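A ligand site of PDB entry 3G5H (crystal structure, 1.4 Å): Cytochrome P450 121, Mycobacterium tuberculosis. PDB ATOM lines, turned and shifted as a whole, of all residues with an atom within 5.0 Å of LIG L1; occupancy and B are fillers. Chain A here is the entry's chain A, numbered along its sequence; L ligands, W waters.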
ATOM      1  N   LEU A  55      17.957 -20.305   3.678  1.00  0.00           N
ATOM      2  CA  LEU A  55      19.309 -20.869   3.639  1.00  0.00           C
ATOM      3  C   LEU A  55      19.968 -20.773   2.261  1.00  0.00           C
ATOM      4  O   LEU A  55      21.181 -20.829   2.155  1.00  0.00           O
ATOM      5  CB  LEU A  55      19.325 -22.313   4.136  1.00  0.00           C
ATOM      6  CG  LEU A  55      18.942 -22.493   5.601  1.00  0.00           C
ATOM      7  CD1 LEU A  55      18.854 -23.974   5.929  1.00  0.00           C
ATOM      8  CD2 LEU A  55      19.960 -21.782   6.507  1.00  0.00           C
ATOM      9  N   MET A  62      25.328 -15.186   7.453  1.00  0.00           N
ATOM     10  CA  MET A  62      25.873 -15.608   8.743  1.00  0.00           C
ATOM     11  C   MET A  62      26.882 -14.574   9.260  1.00  0.00           C
ATOM     12  O   MET A  62      26.806 -14.161  10.403  1.00  0.00           O
ATOM     13  CB  MET A  62      26.520 -17.001   8.667  1.00  0.00           C
ATOM     14  CG  MET A  62      27.376 -17.445   9.897  1.00  0.00           C
ATOM     15  SD  MET A  62      26.528 -17.423  11.533  1.00  0.00           S
ATOM     16  CE  MET A  62      25.646 -18.980  11.381  1.00  0.00           C
ATOM     17  N   ASN A  85      34.089 -17.997   9.638  1.00  0.00           N
ATOM     18  CA  ASN A  85      35.145 -19.029   9.568  1.00  0.00           C
ATOM     19  C   ASN A  85      35.308 -19.662   8.179  1.00  0.00           C
ATOM     20  O   ASN A  85      36.406 -19.640   7.580  1.00  0.00           O
ATOM     21  CB  ASN A  85      34.921 -20.104  10.658  1.00  0.00           C
ATOM     22  CG  ASN A  85      36.123 -21.003  10.875  1.00  0.00           C
ATOM     23  OD1 ASN A  85      37.263 -20.529  10.870  1.00  0.00           O
ATOM     24  ND2 ASN A  85      35.870 -22.282  11.095  1.00  0.00           N
ATOM     25  N   MET A  86      34.240 -20.231   7.644  1.00  0.00           N
ATOM     26  CA  MET A  86      34.373 -20.894   6.349  1.00  0.00           C
ATOM     27  C   MET A  86      34.737 -19.933   5.227  1.00  0.00           C
ATOM     28  O   MET A  86      35.519 -20.283   4.341  1.00  0.00           O
ATOM     29  CB  MET A  86      33.157 -21.746   6.028  1.00  0.00           C
ATOM     30  CG  MET A  86      33.194 -23.097   6.749  1.00  0.00           C
ATOM     31  SD  MET A  86      34.291 -24.391   6.114  1.00  0.00           S
ATOM     32  CE  MET A  86      34.698 -23.600   4.586  1.00  0.00           C
ATOM     33  N   ILE A 102      38.803 -34.106   6.140  1.00  0.00           N
ATOM     34  CA  ILE A 102      37.755 -34.483   7.092  1.00  0.00           C
ATOM     35  C   ILE A 102      36.719 -35.451   6.507  1.00  0.00           C
ATOM     36  O   ILE A 102      35.643 -35.635   7.073  1.00  0.00           O
ATOM     37  CB  ILE A 102      37.085 -33.236   7.740  1.00  0.00           C
ATOM     38  CG1 ILE A 102      36.313 -32.442   6.683  1.00  0.00           C
ATOM     39  CG2 ILE A 102      38.149 -32.365   8.476  1.00  0.00           C
ATOM     40  CD1 ILE A 102      35.415 -31.350   7.261  1.00  0.00           C
ATOM     41  N   HIS A 146      37.882 -37.147  16.241  1.00  0.00           N
ATOM     42  CA  HIS A 146      38.410 -35.863  15.837  1.00  0.00           C
ATOM     43  C   HIS A 146      39.888 -35.686  16.129  1.00  0.00           C
ATOM     44  O   HIS A 146      40.595 -35.022  15.374  1.00  0.00           O
ATOM     45  CB  HIS A 146      37.535 -34.711  16.361  1.00  0.00           C
ATOM     46  CG  HIS A 146      36.242 -34.618  15.605  1.00  0.00           C
ATOM     47  ND1 HIS A 146      35.185 -35.480  15.825  1.00  0.00           N
ATOM     48  CD2 HIS A 146      35.873 -33.822  14.578  1.00  0.00           C
ATOM     49  CE1 HIS A 146      34.213 -35.207  14.965  1.00  0.00           C
ATOM     50  NE2 HIS A 146      34.613 -34.202  14.198  1.00  0.00           N
ATOM     51  N   PHE A 230      37.215 -26.808  13.946  1.00  0.00           N
ATOM     52  CA  PHE A 230      36.803 -28.096  13.392  1.00  0.00           C
ATOM     53  C   PHE A 230      36.700 -29.147  14.488  1.00  0.00           C
ATOM     54  O   PHE A 230      35.772 -29.955  14.485  1.00  0.00           O
ATOM     55  CB  PHE A 230      37.641 -28.519  12.148  1.00  0.00           C
ATOM     56  CG  PHE A 230      37.131 -27.876  10.894  1.00  0.00           C
ATOM     57  CD1 PHE A 230      37.187 -26.484  10.738  1.00  0.00           C
ATOM     58  CD2 PHE A 230      36.487 -28.624   9.900  1.00  0.00           C
ATOM     59  CE1 PHE A 230      36.646 -25.844   9.626  1.00  0.00           C
ATOM     60  CE2 PHE A 230      35.945 -27.995   8.768  1.00  0.00           C
ATOM     61  CZ  PHE A 230      36.038 -26.602   8.629  1.00  0.00           C
ATOM     62  N   ALA A 233      33.260 -27.862  16.544  1.00  0.00           N
ATOM     63  CA  ALA A 233      32.001 -28.052  15.849  1.00  0.00           C
ATOM     64  C   ALA A 233      31.786 -29.542  15.543  1.00  0.00           C
ATOM     65  O   ALA A 233      30.684 -30.083  15.692  1.00  0.00           O
ATOM     66  CB  ALA A 233      31.981 -27.245  14.543  1.00  0.00           C
ATOM     67  N   GLY A 234      32.844 -30.229  15.111  1.00  0.00           N
ATOM     68  CA  GLY A 234      32.707 -31.653  14.799  1.00  0.00           C
ATOM     69  C   GLY A 234      32.388 -32.510  16.034  1.00  0.00           C
ATOM     70  O   GLY A 234      31.493 -33.352  16.006  1.00  0.00           O
ATOM     71  N   SER A 237      28.915 -31.723  17.469  1.00  0.00           N
ATOM     72  CA  SER A 237      27.811 -32.088  16.605  1.00  0.00           C
ATOM     73  C   SER A 237      27.647 -33.599  16.493  1.00  0.00           C
ATOM     74  O   SER A 237      26.533 -34.122  16.593  1.00  0.00           O
ATOM     75  CB  SER A 237      27.984 -31.484  15.212  1.00  0.00           C
ATOM     76  OG  SER A 237      28.037 -30.066  15.296  1.00  0.00           O
ATOM     77  N   THR A 238      28.774 -34.301  16.328  1.00  0.00           N
ATOM     78  CA  THR A 238      28.696 -35.764  16.229  1.00  0.00           C
ATOM     79  C   THR A 238      28.353 -36.416  17.570  1.00  0.00           C
ATOM     80  O   THR A 238      27.530 -37.339  17.630  1.00  0.00           O
ATOM     81  CB  THR A 238      30.005 -36.384  15.674  1.00  0.00           C
ATOM     82  OG1 THR A 238      31.117 -36.000  16.512  1.00  0.00           O
ATOM     83  CG2 THR A 238      30.244 -35.947  14.217  1.00  0.00           C
ATOM     84  N   PHE A 241      24.600 -35.509  18.219  1.00  0.00           N
ATOM     85  CA  PHE A 241      23.709 -36.228  17.337  1.00  0.00           C
ATOM     86  C   PHE A 241      23.657 -37.722  17.679  1.00  0.00           C
ATOM     87  O   PHE A 241      22.567 -38.316  17.794  1.00  0.00           O
ATOM     88  CB  PHE A 241      24.062 -36.064  15.858  1.00  0.00           C
ATOM     89  CG  PHE A 241      23.291 -36.995  15.002  1.00  0.00           C
ATOM     90  CD1 PHE A 241      21.907 -36.902  14.954  1.00  0.00           C
ATOM     91  CD2 PHE A 241      23.912 -38.051  14.321  1.00  0.00           C
ATOM     92  CE1 PHE A 241      21.138 -37.819  14.213  1.00  0.00           C
ATOM     93  CE2 PHE A 241      23.145 -38.954  13.583  1.00  0.00           C
ATOM     94  CZ  PHE A 241      21.778 -38.847  13.532  1.00  0.00           C
ATOM     95  N   LEU A 274      18.834 -38.653  11.431  1.00  0.00           N
ATOM     96  CA  LEU A 274      19.209 -37.258  11.154  1.00  0.00           C
ATOM     97  C   LEU A 274      17.982 -36.402  10.905  1.00  0.00           C
ATOM     98  O   LEU A 274      17.842 -35.306  11.467  1.00  0.00           O
ATOM     99  CB  LEU A 274      20.162 -37.178   9.952  1.00  0.00           C
ATOM    100  CG  LEU A 274      21.591 -37.633  10.245  1.00  0.00           C
ATOM    101  CD1 LEU A 274      22.339 -37.975   8.960  1.00  0.00           C
ATOM    102  CD2 LEU A 274      22.337 -36.541  11.021  1.00  0.00           C
ATOM    103  N   ASN A 277      16.117 -35.552  14.013  1.00  0.00           N
ATOM    104  CA  ASN A 277      16.979 -35.175  15.145  1.00  0.00           C
ATOM    105  C   ASN A 277      16.668 -33.791  15.675  1.00  0.00           C
ATOM    106  O   ASN A 277      16.447 -32.861  14.894  1.00  0.00           O
ATOM    107  CB  ASN A 277      18.474 -35.371  14.816  1.00  0.00           C
ATOM    108  CG  ASN A 277      19.200 -34.085  14.501  1.00  0.00           C
ATOM    109  OD1 ASN A 277      19.588 -33.364  15.415  1.00  0.00           O
ATOM    110  ND2 ASN A 277      19.438 -33.801  13.202  1.00  0.00           N
ATOM    111  N   PHE A 280      19.901 -29.636  17.326  1.00  0.00           N
ATOM    112  CA  PHE A 280      20.117 -28.168  17.304  1.00  0.00           C
ATOM    113  C   PHE A 280      19.078 -27.478  18.159  1.00  0.00           C
ATOM    114  O   PHE A 280      17.889 -27.594  17.906  1.00  0.00           O
ATOM    115  CB  PHE A 280      20.121 -27.615  15.876  1.00  0.00           C
ATOM    116  CG  PHE A 280      21.462 -27.751  15.204  1.00  0.00           C
ATOM    117  CD1 PHE A 280      22.005 -29.001  14.959  1.00  0.00           C
ATOM    118  CD2 PHE A 280      22.189 -26.635  14.867  1.00  0.00           C
ATOM    119  CE1 PHE A 280      23.251 -29.127  14.344  1.00  0.00           C
ATOM    120  CE2 PHE A 280      23.455 -26.770  14.256  1.00  0.00           C
ATOM    121  CZ  PHE A 280      23.974 -28.018  14.012  1.00  0.00           C
ATOM    122  N   LEU A 284      18.939 -21.794  13.028  1.00  0.00           N
ATOM    123  CA  LEU A 284      20.183 -21.267  12.442  1.00  0.00           C
ATOM    124  C   LEU A 284      20.005 -19.779  12.194  1.00  0.00           C
ATOM    125  O   LEU A 284      19.038 -19.366  11.580  1.00  0.00           O
ATOM    126  CB  LEU A 284      20.495 -21.975  11.116  1.00  0.00           C
ATOM    127  CG  LEU A 284      20.611 -23.493  11.207  1.00  0.00           C
ATOM    128  CD1 LEU A 284      20.955 -24.010   9.817  1.00  0.00           C
ATOM    129  CD2 LEU A 284      21.648 -23.961  12.221  1.00  0.00           C
ATOM    130  N   PRO A 285      20.921 -18.951  12.731  1.00  0.00           N
ATOM    131  CA  PRO A 285      20.754 -17.502  12.605  1.00  0.00           C
ATOM    132  C   PRO A 285      21.327 -16.930  11.311  1.00  0.00           C
ATOM    133  O   PRO A 285      22.395 -17.364  10.835  1.00  0.00           O
ATOM    134  CB  PRO A 285      21.547 -16.949  13.792  1.00  0.00           C
ATOM    135  CG  PRO A 285      22.675 -17.937  13.982  1.00  0.00           C
ATOM    136  CD  PRO A 285      22.083 -19.309  13.569  1.00  0.00           C
ATOM    137  N   ARG A 286      20.614 -15.933  10.776  1.00  0.00           N
ATOM    138  CA  ARG A 286      21.079 -15.149   9.628  1.00  0.00           C
ATOM    139  C   ARG A 286      20.619 -13.705   9.844  1.00  0.00           C
ATOM    140  O   ARG A 286      19.538 -13.468  10.370  1.00  0.00           O
ATOM    141  CB  ARG A 286      20.456 -15.667   8.336  1.00  0.00           C
ATOM    142  CG  ARG A 286      20.803 -17.119   7.992  1.00  0.00           C
ATOM    143  CD  ARG A 286      22.253 -17.255   7.564  1.00  0.00           C
ATOM    144  NE  ARG A 286      22.560 -18.576   7.006  1.00  0.00           N
ATOM    145  CZ  ARG A 286      23.001 -19.632   7.702  1.00  0.00           C
ATOM    146  NH1 ARG A 286      23.129 -19.583   9.027  1.00  0.00           N
ATOM    147  NH2 ARG A 286      23.260 -20.771   7.052  1.00  0.00           N
ATOM    148  N   LEU A 309      15.326 -25.917  12.190  1.00  0.00           N
ATOM    149  CA  LEU A 309      15.576 -27.152  11.408  1.00  0.00           C
ATOM    150  C   LEU A 309      14.474 -28.180  11.567  1.00  0.00           C
ATOM    151  O   LEU A 309      14.081 -28.827  10.573  1.00  0.00           O
ATOM    152  CB  LEU A 309      16.943 -27.753  11.768  1.00  0.00           C
ATOM    153  CG  LEU A 309      18.148 -26.871  11.418  1.00  0.00           C
ATOM    154  CD1 LEU A 309      19.462 -27.601  11.724  1.00  0.00           C
ATOM    155  CD2 LEU A 309      18.114 -26.414   9.943  1.00  0.00           C
ATOM    156  N   LEU A 336      17.182 -31.083   6.310  1.00  0.00           N
ATOM    157  CA  LEU A 336      18.093 -29.973   6.591  1.00  0.00           C
ATOM    158  C   LEU A 336      18.971 -30.195   7.823  1.00  0.00           C
ATOM    159  O   LEU A 336      19.486 -29.234   8.410  1.00  0.00           O
ATOM    160  CB  LEU A 336      17.321 -28.660   6.761  1.00  0.00           C
ATOM    161  CG  LEU A 336      16.359 -28.221   5.640  1.00  0.00           C
ATOM    162  CD1 LEU A 336      15.931 -26.777   5.843  1.00  0.00           C
ATOM    163  CD2 LEU A 336      16.945 -28.370   4.257  1.00  0.00           C
ATOM    164  N   ALA A 337      19.197 -31.453   8.203  1.00  0.00           N
ATOM    165  CA  ALA A 337      20.026 -31.716   9.405  1.00  0.00           C
ATOM    166  C   ALA A 337      21.435 -31.185   9.280  1.00  0.00           C
ATOM    167  O   ALA A 337      22.052 -30.884  10.281  1.00  0.00           O
ATOM    168  CB  ALA A 337      20.085 -33.198   9.746  1.00  0.00           C
ATOM    169  N   PHE A 338      21.948 -31.098   8.052  1.00  0.00           N
ATOM    170  CA  PHE A 338      23.287 -30.549   7.797  1.00  0.00           C
ATOM    171  C   PHE A 338      23.219 -29.137   7.219  1.00  0.00           C
ATOM    172  O   PHE A 338      24.197 -28.646   6.681  1.00  0.00           O
ATOM    173  CB  PHE A 338      24.063 -31.465   6.846  1.00  0.00           C
ATOM    174  CG  PHE A 338      24.411 -32.815   7.458  1.00  0.00           C
ATOM    175  CD1 PHE A 338      25.254 -32.894   8.566  1.00  0.00           C
ATOM    176  CD2 PHE A 338      23.945 -34.001   6.890  1.00  0.00           C
ATOM    177  CE1 PHE A 338      25.573 -34.124   9.132  1.00  0.00           C
ATOM    178  CE2 PHE A 338      24.276 -35.222   7.440  1.00  0.00           C
ATOM    179  CZ  PHE A 338      25.083 -35.291   8.551  1.00  0.00           C
ATOM    180  N   GLY A 339      22.050 -28.518   7.311  1.00  0.00           N
ATOM    181  CA  GLY A 339      21.832 -27.200   6.730  1.00  0.00           C
ATOM    182  C   GLY A 339      21.612 -27.314   5.224  1.00  0.00           C
ATOM    183  O   GLY A 339      21.207 -28.369   4.698  1.00  0.00           O
ATOM    184  N   GLN A 342      25.066 -22.133   1.113  1.00  0.00           N
ATOM    185  CA  GLN A 342      26.474 -21.772   1.273  1.00  0.00           C
ATOM    186  C   GLN A 342      27.151 -22.416   2.492  1.00  0.00           C
ATOM    187  O   GLN A 342      28.336 -22.756   2.449  1.00  0.00           O
ATOM    188  CB  GLN A 342      26.607 -20.257   1.339  1.00  0.00           C
ATOM    189  CG  GLN A 342      28.032 -19.727   1.472  1.00  0.00           C
ATOM    190  CD  GLN A 342      28.801 -19.673   0.153  1.00  0.00           C
ATOM    191  OE1 GLN A 342      29.974 -19.285   0.125  1.00  0.00           O
ATOM    192  NE2 GLN A 342      28.142 -20.040  -0.936  1.00  0.00           N
ATOM    193  N   HIS A 343      26.389 -22.555   3.581  1.00  0.00           N
ATOM    194  CA  HIS A 343      26.935 -23.055   4.827  1.00  0.00           C
ATOM    195  C   HIS A 343      26.685 -24.534   5.107  1.00  0.00           C
ATOM    196  O   HIS A 343      26.851 -24.994   6.242  1.00  0.00           O
ATOM    197  CB  HIS A 343      26.426 -22.206   5.998  1.00  0.00           C
ATOM    198  CG  HIS A 343      26.869 -20.784   5.925  1.00  0.00           C
ATOM    199  ND1 HIS A 343      28.062 -20.346   6.448  1.00  0.00           N
ATOM    200  CD2 HIS A 343      26.278 -19.690   5.364  1.00  0.00           C
ATOM    201  CE1 HIS A 343      28.190 -19.048   6.224  1.00  0.00           C
ATOM    202  NE2 HIS A 343      27.136 -18.625   5.561  1.00  0.00           N
ATOM    203  N   PHE A 344      26.309 -25.283   4.069  1.00  0.00           N
ATOM    204  CA  PHE A 344      26.074 -26.707   4.213  1.00  0.00           C
ATOM    205  C   PHE A 344      27.265 -27.348   4.928  1.00  0.00           C
ATOM    206  O   PHE A 344      28.434 -27.095   4.597  1.00  0.00           O
ATOM    207  CB  PHE A 344      25.883 -27.370   2.839  1.00  0.00           C
ATOM    208  CG  PHE A 344      25.565 -28.828   2.931  1.00  0.00           C
ATOM    209  CD1 PHE A 344      24.260 -29.244   3.158  1.00  0.00           C
ATOM    210  CD2 PHE A 344      26.585 -29.800   2.862  1.00  0.00           C
ATOM    211  CE1 PHE A 344      23.950 -30.605   3.269  1.00  0.00           C
ATOM    212  CE2 PHE A 344      26.272 -31.158   2.997  1.00  0.00           C
ATOM    213  CZ  PHE A 344      24.964 -31.547   3.200  1.00  0.00           C
ATOM    214  N   CYS A 345      26.979 -28.177   5.933  1.00  0.00           N
ATOM    215  CA  CYS A 345      28.023 -28.786   6.777  1.00  0.00           C
ATOM    216  C   CYS A 345      29.154 -29.427   5.964  1.00  0.00           C
ATOM    217  O   CYS A 345      28.899 -30.366   5.185  1.00  0.00           O
ATOM    218  CB  CYS A 345      27.402 -29.856   7.679  1.00  0.00           C
ATOM    219  SG  CYS A 345      28.623 -30.593   8.769  1.00  0.00           S
ATOM    220  N   PRO A 346      30.393 -28.968   6.212  1.00  0.00           N
ATOM    221  CA  PRO A 346      31.489 -29.592   5.480  1.00  0.00           C
ATOM    222  C   PRO A 346      31.895 -30.961   6.051  1.00  0.00           C
ATOM    223  O   PRO A 346      32.701 -31.684   5.437  1.00  0.00           O
ATOM    224  CB  PRO A 346      32.628 -28.572   5.637  1.00  0.00           C
ATOM    225  CG  PRO A 346      32.367 -27.976   6.998  1.00  0.00           C
ATOM    226  CD  PRO A 346      30.870 -27.879   7.091  1.00  0.00           C
ATOM    227  N   GLY A 347      31.364 -31.303   7.224  1.00  0.00           N
ATOM    228  CA  GLY A 347      31.659 -32.605   7.841  1.00  0.00           C
ATOM    229  C   GLY A 347      30.562 -33.651   7.684  1.00  0.00           C
ATOM    230  O   GLY A 347      30.578 -34.653   8.404  1.00  0.00           O
ATOM    231  N   LEU A 350      31.485 -37.374   7.310  1.00  0.00           N
ATOM    232  CA  LEU A 350      32.088 -37.863   8.544  1.00  0.00           C
ATOM    233  C   LEU A 350      31.066 -38.048   9.650  1.00  0.00           C
ATOM    234  O   LEU A 350      31.117 -39.029  10.397  1.00  0.00           O
ATOM    235  CB  LEU A 350      33.221 -36.950   8.998  1.00  0.00           C
ATOM    236  CG  LEU A 350      34.098 -37.414  10.170  1.00  0.00           C
ATOM    237  CD1 LEU A 350      34.907 -38.668   9.827  1.00  0.00           C
ATOM    238  CD2 LEU A 350      35.022 -36.291  10.641  1.00  0.00           C
ATOM    239  N   GLY A 351      30.136 -37.106   9.757  1.00  0.00           N
ATOM    240  CA  GLY A 351      29.074 -37.210  10.763  1.00  0.00           C
ATOM    241  C   GLY A 351      28.210 -38.427  10.524  1.00  0.00           C
ATOM    242  O   GLY A 351      27.876 -39.160  11.467  1.00  0.00           O
HETATM  243  C1  LIG L   1      27.922 -26.334   9.708  1.00  0.00           C
HETATM  244  C2  LIG L   1      25.148 -29.953  11.440  1.00  0.00           C
HETATM  245  C3  LIG L   1      29.170 -32.676  11.903  1.00  0.00           C
HETATM  246  C4  LIG L   1      31.925 -28.799  11.041  1.00  0.00           C
HETATM  247  C5  LIG L   1      26.825 -27.093  10.043  1.00  0.00           C
HETATM  248  C6  LIG L   1      25.438 -26.715   9.905  1.00  0.00           C
HETATM  249  C7  LIG L   1      24.669 -27.714  10.402  1.00  0.00           C
HETATM  250  C8  LIG L   1      25.551 -28.762  10.863  1.00  0.00           C
HETATM  251  C9  LIG L   1      23.121 -27.743  10.494  1.00  0.00           C
HETATM  252  C10 LIG L   1      24.939 -25.392   9.275  1.00  0.00           C
HETATM  253  C11 LIG L   1      25.019 -24.216  10.217  1.00  0.00           C
HETATM  254  C12 LIG L   1      24.438 -22.984   9.571  1.00  0.00           C
HETATM  255  O1  LIG L   1      24.080 -22.991   8.355  1.00  0.00           O
HETATM  256  O2  LIG L   1      24.351 -21.957  10.312  1.00  0.00           O
HETATM  257  C13 LIG L   1      26.009 -31.002  11.726  1.00  0.00           C
HETATM  258  C14 LIG L   1      25.603 -32.322  12.189  1.00  0.00           C
HETATM  259  C15 LIG L   1      26.727 -33.073  12.314  1.00  0.00           C
HETATM  260  C16 LIG L   1      27.865 -32.248  11.955  1.00  0.00           C
HETATM  261  C17 LIG L   1      24.135 -32.744  12.443  1.00  0.00           C
HETATM  262  C18 LIG L   1      26.854 -34.545  12.762  1.00  0.00           C
HETATM  263  C19 LIG L   1      25.865 -35.444  12.654  1.00  0.00           C
HETATM  264  C20 LIG L   1      30.252 -31.894  11.638  1.00  0.00           C
HETATM  265  C21 LIG L   1      31.642 -32.336  11.581  1.00  0.00           C
HETATM  266  C22 LIG L   1      32.409 -31.253  11.360  1.00  0.00           C
HETATM  267  C23 LIG L   1      31.532 -30.109  11.223  1.00  0.00           C
HETATM  268  C24 LIG L   1      32.084 -33.815  11.776  1.00  0.00           C
HETATM  269  C25 LIG L   1      33.944 -31.141  11.219  1.00  0.00           C
HETATM  270  C26 LIG L   1      34.825 -32.097  11.505  1.00  0.00           C
HETATM  271  C27 LIG L   1      31.114 -27.777  10.648  1.00  0.00           C
HETATM  272  C28 LIG L   1      31.563 -26.448  10.309  1.00  0.00           C
HETATM  273  C29 LIG L   1      30.327 -25.699   9.869  1.00  0.00           C
HETATM  274  C30 LIG L   1      29.230 -26.617  10.020  1.00  0.00           C
HETATM  275  C31 LIG L   1      32.989 -25.907  10.350  1.00  0.00           C
HETATM  276  C32 LIG L   1      30.245 -24.248   9.363  1.00  0.00           C
HETATM  277  C33 LIG L   1      30.154 -24.333   7.836  1.00  0.00           C
HETATM  278  C34 LIG L   1      29.944 -23.003   7.151  1.00  0.00           C
HETATM  279  O3  LIG L   1      30.022 -22.963   5.873  1.00  0.00           O
HETATM  280  O4  LIG L   1      29.688 -22.013   7.861  1.00  0.00           O
HETATM  281  N1  LIG L   1      26.870 -28.357  10.610  1.00  0.00           N
HETATM  282  N2  LIG L   1      27.400 -30.991  11.646  1.00  0.00           N
HETATM  283  N3  LIG L   1      30.228 -30.535  11.389  1.00  0.00           N
HETATM  284  N4  LIG L   1      29.730 -27.837  10.494  1.00  0.00           N
HETATM  285 FE1  LIG L   1      28.550 -29.510  10.846  1.00  0.00          FE
HETATM  286  O1  LG2 L   2      33.054 -22.758  11.931  1.00  0.00           O
HETATM  287  C1  LG2 L   2      32.462 -21.876  12.564  1.00  0.00           C
HETATM  288  C2  LG2 L   2      32.579 -21.810  14.063  1.00  0.00           C
HETATM  289  C3  LG2 L   2      31.914 -23.024  14.761  1.00  0.00           C
HETATM  290  C4  LG2 L   2      32.409 -23.007  16.198  1.00  0.00           C
HETATM  291  C5  LG2 L   2      33.570 -23.683  16.555  1.00  0.00           C
HETATM  292  C6  LG2 L   2      34.084 -23.622  17.865  1.00  0.00           C
HETATM  293  C7  LG2 L   2      33.382 -22.868  18.835  1.00  0.00           C
HETATM  294  O2  LG2 L   2      33.863 -22.796  20.107  1.00  0.00           O
HETATM  295  C8  LG2 L   2      32.197 -22.207  18.494  1.00  0.00           C
HETATM  296  C9  LG2 L   2      31.711 -22.277  17.175  1.00  0.00           C
HETATM  297  N1  LG2 L   2      32.067 -20.551  14.621  1.00  0.00           N
HETATM  298  N2  LG2 L   2      31.723 -20.958  11.931  1.00  0.00           N
HETATM  299  C10 LG2 L   2      30.926 -19.903  12.545  1.00  0.00           C
HETATM  300  C11 LG2 L   2      31.266 -19.687  13.991  1.00  0.00           C
HETATM  301  O3  LG2 L   2      30.781 -18.705  14.547  1.00  0.00           O
HETATM  302  C12 LG2 L   2      29.417 -20.178  12.364  1.00  0.00           C
HETATM  303  C13 LG2 L   2      28.961 -21.442  13.076  1.00  0.00           C
HETATM  304  C14 LG2 L   2      28.496 -21.376  14.392  1.00  0.00           C
HETATM  305  C15 LG2 L   2      28.094 -22.544  15.032  1.00  0.00           C
HETATM  306  C16 LG2 L   2      28.120 -23.784  14.374  1.00  0.00           C
HETATM  307  O4  LG2 L   2      27.736 -24.924  15.014  1.00  0.00           O
HETATM  308  C17 LG2 L   2      28.596 -23.857  13.056  1.00  0.00           C
HETATM  309  C18 LG2 L   2      29.000 -22.679  12.436  1.00  0.00           C
HETATM  310  O   HOH W   1      30.212 -20.919   4.099  1.00  0.00           O
HETATM  311  O   HOH W   2      23.477 -24.383   6.161  1.00  0.00           O
HETATM  312  O   HOH W   3      31.619 -20.582   9.047  1.00  0.00           O
HETATM  313  O   HOH W   4      26.944 -26.747  13.405  1.00  0.00           O
HETATM  314  O   HOH W   5      30.455 -25.197   4.495  1.00  0.00           O
HETATM  315  O   HOH W   6      28.537 -28.527  13.077  1.00  0.00           O
HETATM  316  O   HOH W   7      25.312 -22.014  12.846  1.00  0.00           O
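FE1 of LIG L1 is bound by SG of Cys 345 (2.3 Å).
NH2 of Arg 286 is in salt-bridge range of O1 of LIG L1, 2.7 Å away.
An oxygen (O4) of LIG L1 lies within hydrogen-bond range of a ring nitrogen (ND1) of His 343 (2.7 Å).
ND2 of Asn 85 is in hydrogen-bond range of O1 of LG2 L2, at 3.0 Å.
The backbone NH (N) of Cys 345 is in hydrogen-bond range of the backbone carbonyl oxygen (O) of Phe 338, 2.9 Å away.
SG of Cys 345 lies close to N of Gly 347 (3.2 Å).
The side-chain hydroxyl (OG) of Ser 237 is in hydrogen-bond range of the backbone carbonyl oxygen (O) of Ala 233, at 2.7 Å.
O of Gly 234 sits at hydrogen-bond distance from OG1 of Thr 238.
Met 62 touches LIG L1.
Met 86 touches LIG L1.
His 146 touches LIG L1.
Phe 230 touches LIG L1 (CZ to C31, 3.6 Å).
CB of Ala 233 touches C4 of LIG L1, 3.8 Å away.
Gly 234 touches LIG L1.
Ser 237 touches LIG L1.
Thr 238 touches LIG L1.
Phe 241 touches LIG L1 (CD2 to C19, 3.7 Å).
Phe 280 touches LIG L1.
Leu 284 touches LIG L1 (CD1 to O1, 3.6 Å).
CD1 of Leu 309 touches C9 of LIG L1, at 3.9 Å.
O of Ala 337 touches C9 of LIG L1, at 3.3 Å.
CE1 of Phe 338 touches C15 of LIG L1, at 3.5 Å.
N of Gly 339 touches C9 of LIG L1, 3.4 Å away.
Gln 342 touches LIG L1.
Pro 346 touches LIG L1 (CD to C27, 3.6 Å).
Gly 347 touches LIG L1.
Hydrophobic or aromatic side chains within 4 Å of LIG L1: Met 62, Met 86, His 146, Phe 230, Ala 233, Phe 241, Phe 280, Leu 284, Leu 309, Phe 338, His 343 and Pro 346.
21 residues have an atom within 4 Å of LIG L1: Met 62, Met 86, His 146, Phe 230, Ala 233, Gly 234, Ser 237, Thr 238, Phe 241, Phe 280, Leu 284, Arg 286, Leu 309, Ala 337, Phe 338, Gly 339, Gln 342, His 343, Cys 345, Pro 346 and Gly 347.
Water W5 bridges O3 of LIG L1 (2.7 Å) and O of Phe 344 (2.8 Å).
Water W2 bridges O1 of LIG L1 and O of His 343.
Water W3 lies within hydrogen-bond range of an oxygen (O4) of LIG L1 (2.7 Å), a nitrogen (N2) of LG2 L2 (2.9 Å) and the backbone NH (N) of Met 86 (3.0 Å).
Water W1 lies within hydrogen-bond range of an oxygen (O3) of LIG L1 (2.7 Å), the backbone carbonyl oxygen of Gln 342 (3.1 Å) and a ring nitrogen (ND1) of His 343 (3.2 Å).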
